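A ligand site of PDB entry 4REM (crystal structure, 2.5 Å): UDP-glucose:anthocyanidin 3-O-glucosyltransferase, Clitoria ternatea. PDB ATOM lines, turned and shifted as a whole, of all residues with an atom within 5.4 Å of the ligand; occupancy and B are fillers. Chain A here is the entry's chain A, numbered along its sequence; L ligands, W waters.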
ATOM      1  N   PHE A  12      -6.107 -11.846  35.958  1.00  0.00           N
ATOM      2  CA  PHE A  12      -6.828 -10.623  35.684  1.00  0.00           C
ATOM      3  C   PHE A  12      -8.265 -11.080  35.531  1.00  0.00           C
ATOM      4  O   PHE A  12      -8.627 -11.674  34.513  1.00  0.00           O
ATOM      5  CB  PHE A  12      -6.308  -9.962  34.408  1.00  0.00           C
ATOM      6  CG  PHE A  12      -6.739  -8.524  34.245  1.00  0.00           C
ATOM      7  CD1 PHE A  12      -6.573  -7.612  35.277  1.00  0.00           C
ATOM      8  CD2 PHE A  12      -7.271  -8.089  33.049  1.00  0.00           C
ATOM      9  CE1 PHE A  12      -6.956  -6.301  35.125  1.00  0.00           C
ATOM     10  CE2 PHE A  12      -7.657  -6.771  32.890  1.00  0.00           C
ATOM     11  CZ  PHE A  12      -7.497  -5.869  33.928  1.00  0.00           C
ATOM     12  N   PHE A  14     -11.135 -11.086  34.411  1.00  0.00           N
ATOM     13  CA  PHE A  14     -12.061 -10.641  33.379  1.00  0.00           C
ATOM     14  C   PHE A  14     -11.974 -11.465  32.099  1.00  0.00           C
ATOM     15  O   PHE A  14     -10.882 -11.677  31.561  1.00  0.00           O
ATOM     16  CB  PHE A  14     -11.818  -9.160  33.050  1.00  0.00           C
ATOM     17  CG  PHE A  14     -11.859  -8.249  34.238  1.00  0.00           C
ATOM     18  CD1 PHE A  14     -13.066  -7.757  34.716  1.00  0.00           C
ATOM     19  CD2 PHE A  14     -10.685  -7.874  34.881  1.00  0.00           C
ATOM     20  CE1 PHE A  14     -13.101  -6.911  35.813  1.00  0.00           C
ATOM     21  CE2 PHE A  14     -10.720  -7.029  35.979  1.00  0.00           C
ATOM     22  CZ  PHE A  14     -11.922  -6.549  36.441  1.00  0.00           C
ATOM     23  N   GLY A  15     -13.133 -11.926  31.633  1.00  0.00           N
ATOM     24  CA  GLY A  15     -13.298 -12.564  30.334  1.00  0.00           C
ATOM     25  C   GLY A  15     -12.157 -13.384  29.763  1.00  0.00           C
ATOM     26  O   GLY A  15     -11.834 -14.453  30.271  1.00  0.00           O
ATOM     27  N   SER A  16     -11.535 -12.870  28.701  1.00  0.00           N
ATOM     28  CA  SER A  16     -10.555 -13.612  27.924  1.00  0.00           C
ATOM     29  C   SER A  16      -9.217 -13.848  28.626  1.00  0.00           C
ATOM     30  O   SER A  16      -8.370 -14.574  28.121  1.00  0.00           O
ATOM     31  CB  SER A  16     -10.313 -12.921  26.573  1.00  0.00           C
ATOM     32  OG  SER A  16      -9.831 -11.607  26.753  1.00  0.00           O
ATOM     33  N   HIS A  17      -9.029 -13.228  29.789  1.00  0.00           N
ATOM     34  CA  HIS A  17      -7.807 -13.416  30.559  1.00  0.00           C
ATOM     35  C   HIS A  17      -7.891 -14.658  31.450  1.00  0.00           C
ATOM     36  O   HIS A  17      -6.882 -15.187  31.892  1.00  0.00           O
ATOM     37  CB  HIS A  17      -7.520 -12.185  31.435  1.00  0.00           C
ATOM     38  CG  HIS A  17      -6.949 -11.027  30.679  1.00  0.00           C
ATOM     39  ND1 HIS A  17      -5.610 -10.696  30.728  1.00  0.00           N
ATOM     40  CD2 HIS A  17      -7.530 -10.099  29.882  1.00  0.00           C
ATOM     41  CE1 HIS A  17      -5.393  -9.621  29.986  1.00  0.00           C
ATOM     42  NE2 HIS A  17      -6.545  -9.245  29.460  1.00  0.00           N
ATOM     43  N   PRO A  78     -15.934  -0.582  29.379  1.00  0.00           N
ATOM     44  CA  PRO A  78     -15.169  -1.789  29.747  1.00  0.00           C
ATOM     45  C   PRO A  78     -13.938  -1.527  30.614  1.00  0.00           C
ATOM     46  O   PRO A  78     -13.217  -2.473  30.934  1.00  0.00           O
ATOM     47  CB  PRO A  78     -14.742  -2.347  28.384  1.00  0.00           C
ATOM     48  CG  PRO A  78     -14.730  -1.169  27.480  1.00  0.00           C
ATOM     49  CD  PRO A  78     -15.883  -0.335  27.932  1.00  0.00           C
ATOM     50  N   ILE A  79     -13.708  -0.273  30.995  1.00  0.00           N
ATOM     51  CA  ILE A  79     -12.531   0.083  31.771  1.00  0.00           C
ATOM     52  C   ILE A  79     -12.820   0.180  33.278  1.00  0.00           C
ATOM     53  O   ILE A  79     -11.977  -0.143  34.108  1.00  0.00           O
ATOM     54  CB  ILE A  79     -11.912   1.403  31.271  1.00  0.00           C
ATOM     55  CG1 ILE A  79     -11.606   1.319  29.772  1.00  0.00           C
ATOM     56  CG2 ILE A  79     -10.662   1.764  32.054  1.00  0.00           C
ATOM     57  CD1 ILE A  79     -10.608   0.235  29.427  1.00  0.00           C
ATOM     58  N   LEU A  82     -12.316  -2.823  35.552  1.00  0.00           N
ATOM     59  CA  LEU A  82     -10.895  -3.107  35.611  1.00  0.00           C
ATOM     60  C   LEU A  82     -10.222  -2.174  36.623  1.00  0.00           C
ATOM     61  O   LEU A  82      -9.428  -2.622  37.456  1.00  0.00           O
ATOM     62  CB  LEU A  82     -10.242  -2.933  34.234  1.00  0.00           C
ATOM     63  CG  LEU A  82     -10.971  -3.472  33.001  1.00  0.00           C
ATOM     64  CD1 LEU A  82     -10.148  -3.192  31.755  1.00  0.00           C
ATOM     65  CD2 LEU A  82     -11.275  -4.943  33.119  1.00  0.00           C
ATOM     66  N   PHE A 116      -0.993  -7.919  34.372  1.00  0.00           N
ATOM     67  CA  PHE A 116      -1.768  -6.715  34.672  1.00  0.00           C
ATOM     68  C   PHE A 116      -1.966  -6.522  36.173  1.00  0.00           C
ATOM     69  O   PHE A 116      -2.129  -5.396  36.642  1.00  0.00           O
ATOM     70  CB  PHE A 116      -3.122  -6.749  33.953  1.00  0.00           C
ATOM     71  CG  PHE A 116      -3.038  -6.560  32.458  1.00  0.00           C
ATOM     72  CD1 PHE A 116      -1.822  -6.300  31.841  1.00  0.00           C
ATOM     73  CD2 PHE A 116      -4.178  -6.644  31.677  1.00  0.00           C
ATOM     74  CE1 PHE A 116      -1.743  -6.132  30.464  1.00  0.00           C
ATOM     75  CE2 PHE A 116      -4.110  -6.480  30.300  1.00  0.00           C
ATOM     76  CZ  PHE A 116      -2.903  -6.224  29.697  1.00  0.00           C
ATOM     77  N   TRP A 135       1.431 -13.761  30.372  1.00  0.00           N
ATOM     78  CA  TRP A 135       1.105 -12.832  29.291  1.00  0.00           C
ATOM     79  C   TRP A 135       0.237 -13.468  28.205  1.00  0.00           C
ATOM     80  O   TRP A 135       0.749 -14.093  27.276  1.00  0.00           O
ATOM     81  CB  TRP A 135       2.392 -12.279  28.679  1.00  0.00           C
ATOM     82  CG  TRP A 135       2.174 -11.140  27.744  1.00  0.00           C
ATOM     83  CD1 TRP A 135       2.111 -11.195  26.390  1.00  0.00           C
ATOM     84  CD2 TRP A 135       1.987  -9.771  28.107  1.00  0.00           C
ATOM     85  NE1 TRP A 135       1.899  -9.939  25.877  1.00  0.00           N
ATOM     86  CE2 TRP A 135       1.823  -9.036  26.916  1.00  0.00           C
ATOM     87  CE3 TRP A 135       1.953  -9.080  29.326  1.00  0.00           C
ATOM     88  CZ2 TRP A 135       1.625  -7.660  26.904  1.00  0.00           C
ATOM     89  CZ3 TRP A 135       1.757  -7.710  29.306  1.00  0.00           C
ATOM     90  CH2 TRP A 135       1.587  -7.015  28.104  1.00  0.00           C
ATOM     91  N   ASN A 137      -1.724 -11.729  26.218  1.00  0.00           N
ATOM     92  CA  ASN A 137      -2.010 -10.716  25.215  1.00  0.00           C
ATOM     93  C   ASN A 137      -1.192 -10.959  23.943  1.00  0.00           C
ATOM     94  O   ASN A 137      -0.539 -11.997  23.815  1.00  0.00           O
ATOM     95  CB  ASN A 137      -1.719  -9.326  25.771  1.00  0.00           C
ATOM     96  CG  ASN A 137      -2.308  -9.135  27.159  1.00  0.00           C
ATOM     97  OD1 ASN A 137      -1.583  -8.900  28.131  1.00  0.00           O
ATOM     98  ND2 ASN A 137      -3.624  -9.228  27.272  1.00  0.00           N
ATOM     99  N   VAL A 138      -1.231 -10.010  23.020  1.00  0.00           N
ATOM    100  CA  VAL A 138      -0.372 -10.085  21.827  1.00  0.00           C
ATOM    101  C   VAL A 138       1.088 -10.056  22.283  1.00  0.00           C
ATOM    102  O   VAL A 138       1.505  -9.123  22.962  1.00  0.00           O
ATOM    103  CB  VAL A 138      -0.640  -8.923  20.844  1.00  0.00           C
ATOM    104  CG1 VAL A 138       0.308  -8.981  19.667  1.00  0.00           C
ATOM    105  CG2 VAL A 138      -2.075  -8.962  20.352  1.00  0.00           C
ATOM    106  N   SER A 141       3.619  -7.183  21.564  1.00  0.00           N
ATOM    107  CA  SER A 141       3.321  -5.913  22.231  1.00  0.00           C
ATOM    108  C   SER A 141       4.113  -5.742  23.523  1.00  0.00           C
ATOM    109  O   SER A 141       4.085  -4.676  24.136  1.00  0.00           O
ATOM    110  CB  SER A 141       1.821  -5.788  22.506  1.00  0.00           C
ATOM    111  OG  SER A 141       1.372  -6.824  23.351  1.00  0.00           O
ATOM    112  N   TYR A 145       6.268  -1.629  25.854  1.00  0.00           N
ATOM    113  CA  TYR A 145       6.283  -1.108  27.221  1.00  0.00           C
ATOM    114  C   TYR A 145       7.684  -0.757  27.734  1.00  0.00           C
ATOM    115  O   TYR A 145       7.828  -0.215  28.825  1.00  0.00           O
ATOM    116  CB  TYR A 145       5.573  -2.085  28.157  1.00  0.00           C
ATOM    117  CG  TYR A 145       4.131  -2.309  27.754  1.00  0.00           C
ATOM    118  CD1 TYR A 145       3.157  -1.370  28.052  1.00  0.00           C
ATOM    119  CD2 TYR A 145       3.752  -3.455  27.071  1.00  0.00           C
ATOM    120  CE1 TYR A 145       1.851  -1.561  27.681  1.00  0.00           C
ATOM    121  CE2 TYR A 145       2.427  -3.653  26.699  1.00  0.00           C
ATOM    122  CZ  TYR A 145       1.491  -2.702  27.012  1.00  0.00           C
ATOM    123  OH  TYR A 145       0.170  -2.883  26.642  1.00  0.00           O
ATOM    124  N   PRO A 179      -1.209   1.270  20.850  1.00  0.00           N
ATOM    125  CA  PRO A 179      -2.369   1.348  21.746  1.00  0.00           C
ATOM    126  C   PRO A 179      -2.591   2.764  22.284  1.00  0.00           C
ATOM    127  O   PRO A 179      -1.644   3.386  22.764  1.00  0.00           O
ATOM    128  CB  PRO A 179      -1.980   0.413  22.904  1.00  0.00           C
ATOM    129  CG  PRO A 179      -1.025  -0.559  22.299  1.00  0.00           C
ATOM    130  CD  PRO A 179      -0.266   0.210  21.266  1.00  0.00           C
ATOM    131  N   ASP A 181      -4.246   4.086  24.916  1.00  0.00           N
ATOM    132  CA  ASP A 181      -4.072   4.350  26.352  1.00  0.00           C
ATOM    133  C   ASP A 181      -2.601   4.441  26.763  1.00  0.00           C
ATOM    134  O   ASP A 181      -2.290   4.878  27.874  1.00  0.00           O
ATOM    135  CB  ASP A 181      -4.835   3.323  27.205  1.00  0.00           C
ATOM    136  CG  ASP A 181      -4.569   1.890  26.786  1.00  0.00           C
ATOM    137  OD1 ASP A 181      -5.529   1.089  26.808  1.00  0.00           O
ATOM    138  OD2 ASP A 181      -3.417   1.561  26.451  1.00  0.00           O
ATOM    139  N   PHE A 192      -6.019   1.684  34.897  1.00  0.00           N
ATOM    140  CA  PHE A 192      -5.689   0.574  34.025  1.00  0.00           C
ATOM    141  C   PHE A 192      -4.505   0.917  33.110  1.00  0.00           C
ATOM    142  O   PHE A 192      -3.588   0.117  32.960  1.00  0.00           O
ATOM    143  CB  PHE A 192      -6.905   0.186  33.182  1.00  0.00           C
ATOM    144  CG  PHE A 192      -6.661  -0.975  32.255  1.00  0.00           C
ATOM    145  CD1 PHE A 192      -6.299  -2.203  32.756  1.00  0.00           C
ATOM    146  CD2 PHE A 192      -6.816  -0.813  30.885  1.00  0.00           C
ATOM    147  CE1 PHE A 192      -6.068  -3.276  31.900  1.00  0.00           C
ATOM    148  CE2 PHE A 192      -6.600  -1.876  30.031  1.00  0.00           C
ATOM    149  CZ  PHE A 192      -6.226  -3.108  30.538  1.00  0.00           C
ATOM    150  N   LEU A 196      -0.623  -0.567  32.946  1.00  0.00           N
ATOM    151  CA  LEU A 196      -0.009  -1.098  31.742  1.00  0.00           C
ATOM    152  C   LEU A 196       1.295  -0.359  31.409  1.00  0.00           C
ATOM    153  O   LEU A 196       2.255  -0.962  30.936  1.00  0.00           O
ATOM    154  CB  LEU A 196      -0.976  -1.012  30.557  1.00  0.00           C
ATOM    155  CG  LEU A 196      -1.798  -2.261  30.241  1.00  0.00           C
ATOM    156  CD1 LEU A 196      -2.519  -2.781  31.459  1.00  0.00           C
ATOM    157  CD2 LEU A 196      -2.789  -1.977  29.131  1.00  0.00           C
ATOM    158  N   VAL A 274     -16.143  -7.894  24.157  1.00  0.00           N
ATOM    159  CA  VAL A 274     -15.836  -6.613  24.803  1.00  0.00           C
ATOM    160  C   VAL A 274     -16.148  -5.475  23.826  1.00  0.00           C
ATOM    161  O   VAL A 274     -16.563  -4.386  24.228  1.00  0.00           O
ATOM    162  CB  VAL A 274     -14.351  -6.532  25.214  1.00  0.00           C
ATOM    163  CG1 VAL A 274     -14.033  -5.193  25.858  1.00  0.00           C
ATOM    164  CG2 VAL A 274     -14.005  -7.669  26.163  1.00  0.00           C
ATOM    165  N   PHE A 365      -9.221  -1.627  19.712  1.00  0.00           N
ATOM    166  CA  PHE A 365      -8.487  -1.005  20.817  1.00  0.00           C
ATOM    167  C   PHE A 365      -7.329  -1.874  21.285  1.00  0.00           C
ATOM    168  O   PHE A 365      -7.069  -2.941  20.736  1.00  0.00           O
ATOM    169  CB  PHE A 365      -9.424  -0.723  21.993  1.00  0.00           C
ATOM    170  CG  PHE A 365      -9.969  -1.968  22.642  1.00  0.00           C
ATOM    171  CD1 PHE A 365      -9.386  -2.480  23.796  1.00  0.00           C
ATOM    172  CD2 PHE A 365     -11.062  -2.625  22.102  1.00  0.00           C
ATOM    173  CE1 PHE A 365      -9.882  -3.626  24.397  1.00  0.00           C
ATOM    174  CE2 PHE A 365     -11.558  -3.771  22.703  1.00  0.00           C
ATOM    175  CZ  PHE A 365     -10.970  -4.264  23.844  1.00  0.00           C
ATOM    176  N   GLY A 366      -6.634  -1.398  22.321  1.00  0.00           N
ATOM    177  CA  GLY A 366      -5.559  -2.145  22.942  1.00  0.00           C
ATOM    178  C   GLY A 366      -4.436  -2.546  22.011  1.00  0.00           C
ATOM    179  O   GLY A 366      -3.893  -1.713  21.290  1.00  0.00           O
ATOM    180  N   ASP A 367      -4.101  -3.833  22.038  1.00  0.00           N
ATOM    181  CA  ASP A 367      -3.010  -4.354  21.217  1.00  0.00           C
ATOM    182  C   ASP A 367      -3.534  -5.097  19.987  1.00  0.00           C
ATOM    183  O   ASP A 367      -2.829  -5.923  19.409  1.00  0.00           O
ATOM    184  CB  ASP A 367      -2.109  -5.255  22.059  1.00  0.00           C
ATOM    185  CG  ASP A 367      -2.854  -6.421  22.673  1.00  0.00           C
ATOM    186  OD1 ASP A 367      -4.097  -6.415  22.653  1.00  0.00           O
ATOM    187  OD2 ASP A 367      -2.193  -7.339  23.187  1.00  0.00           O
HETATM  188  O1  LIG L   1      -6.936  -3.938  27.192  1.00  0.00           O
HETATM  189  C1  LIG L   1      -7.458  -5.160  27.517  1.00  0.00           C
HETATM  190  C2  LIG L   1      -8.849  -5.176  28.056  1.00  0.00           C
HETATM  191  C3  LIG L   1      -9.430  -6.319  28.601  1.00  0.00           C
HETATM  192  C4  LIG L   1      -3.022  -3.546  25.641  1.00  0.00           C
HETATM  193  C5  LIG L   1      -3.465  -4.835  25.938  1.00  0.00           C
HETATM  194  O2  LIG L   1     -11.287  -7.438  29.639  1.00  0.00           O
HETATM  195  O3  LIG L   1     -11.519  -2.670  28.395  1.00  0.00           O
HETATM  196  C6  LIG L   1      -4.836  -5.018  26.484  1.00  0.00           C
HETATM  197  C7  LIG L   1     -10.858  -3.859  28.466  1.00  0.00           C
HETATM  198  C8  LIG L   1      -9.549  -3.972  28.001  1.00  0.00           C
HETATM  199  C9  LIG L   1     -11.508  -5.049  29.063  1.00  0.00           C
HETATM  200  O4  LIG L   1     -12.790  -4.979  29.532  1.00  0.00           O
HETATM  201  C10 LIG L   1     -10.735  -6.307  29.107  1.00  0.00           C
HETATM  202  C11 LIG L   1      -6.621  -6.395  27.314  1.00  0.00           C
HETATM  203  O5  LIG L   1      -7.081  -7.637  27.609  1.00  0.00           O
HETATM  204  C12 LIG L   1      -5.333  -6.277  26.805  1.00  0.00           C
HETATM  205  C13 LIG L   1      -5.672  -3.815  26.698  1.00  0.00           C
HETATM  206  C14 LIG L   1      -5.139  -2.565  26.369  1.00  0.00           C
HETATM  207  C15 LIG L   1      -3.854  -2.439  25.854  1.00  0.00           C
HETATM  208  O6  LIG L   1      -3.384  -1.194  25.560  1.00  0.00           O
HETATM  209  O7  LIG L   1      -2.648  -5.902  25.729  1.00  0.00           O
HETATM  210  O   HOH W   1      -0.889  -0.683  26.398  1.00  0.00           O
HETATM  211  O   HOH W   2     -11.364  -9.824  28.816  1.00  0.00           O
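An oxygen (O5) of the ligand lies within hydrogen-bond range of a ring nitrogen (NE2) of His 17, 2.5 Å away.
The side-chain carboxylate of Asp 181 is in hydrogen-bond range of an oxygen (O6) of the ligand, at 2.9 Å.
An oxygen (O4) of the ligand is in hydrogen-bond range of the backbone carbonyl oxygen (O) of Pro 78 (2.9 Å).
OD2 of Asp 367 is in hydrogen-bond range of O7 of the ligand (3.0 Å).
The backbone NH of Val 138 is in hydrogen-bond range of the side-chain carboxylate of Asp 367 (2.8 Å).
Phe 14 touches the ligand (CB to O2, 3.9 Å).
Ile 79 touches the ligand (CD1 to O3, 3.2 Å).
Leu 82 touches the ligand (CD1 to C7, 3.4 Å).
Phe 116 touches the ligand.
Asn 137 touches the ligand (ND2 to C12, 3.4 Å).
OH of Tyr 145 touches C4 of the ligand, at 3.4 Å.
CB of Pro 179 touches O6 of the ligand, at 3.4 Å.
Phe 192 touches the ligand (CZ to O1, 3.5 Å).
Leu 196 touches the ligand.
Val 274 touches the ligand.
Phe 365 touches the ligand (CE1 to C8, 3.6 Å).
CA of Gly 366 touches C15 of the ligand, 3.4 Å away.
Hydrophobic or aromatic side chains within 4 Å of the ligand: Phe 14, His 17, Pro 78, Ile 79, Leu 82, Phe 116, Pro 179, Phe 192, Leu 196, Val 274 and Phe 365.
The nearest printed residue that does not touch the ligand is Phe 12 (4.7 Å).
Water W2 lies within hydrogen-bond range of O2 of the ligand (2.5 Å), N of Ser 16 (3.1 Å) and O of Phe 14 (3.3 Å).
Water W1 lies within hydrogen-bond range of OH of Tyr 145 (2.5 Å), O6 of the ligand (2.7 Å) and OD2 of Asp 181 (3.4 Å).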
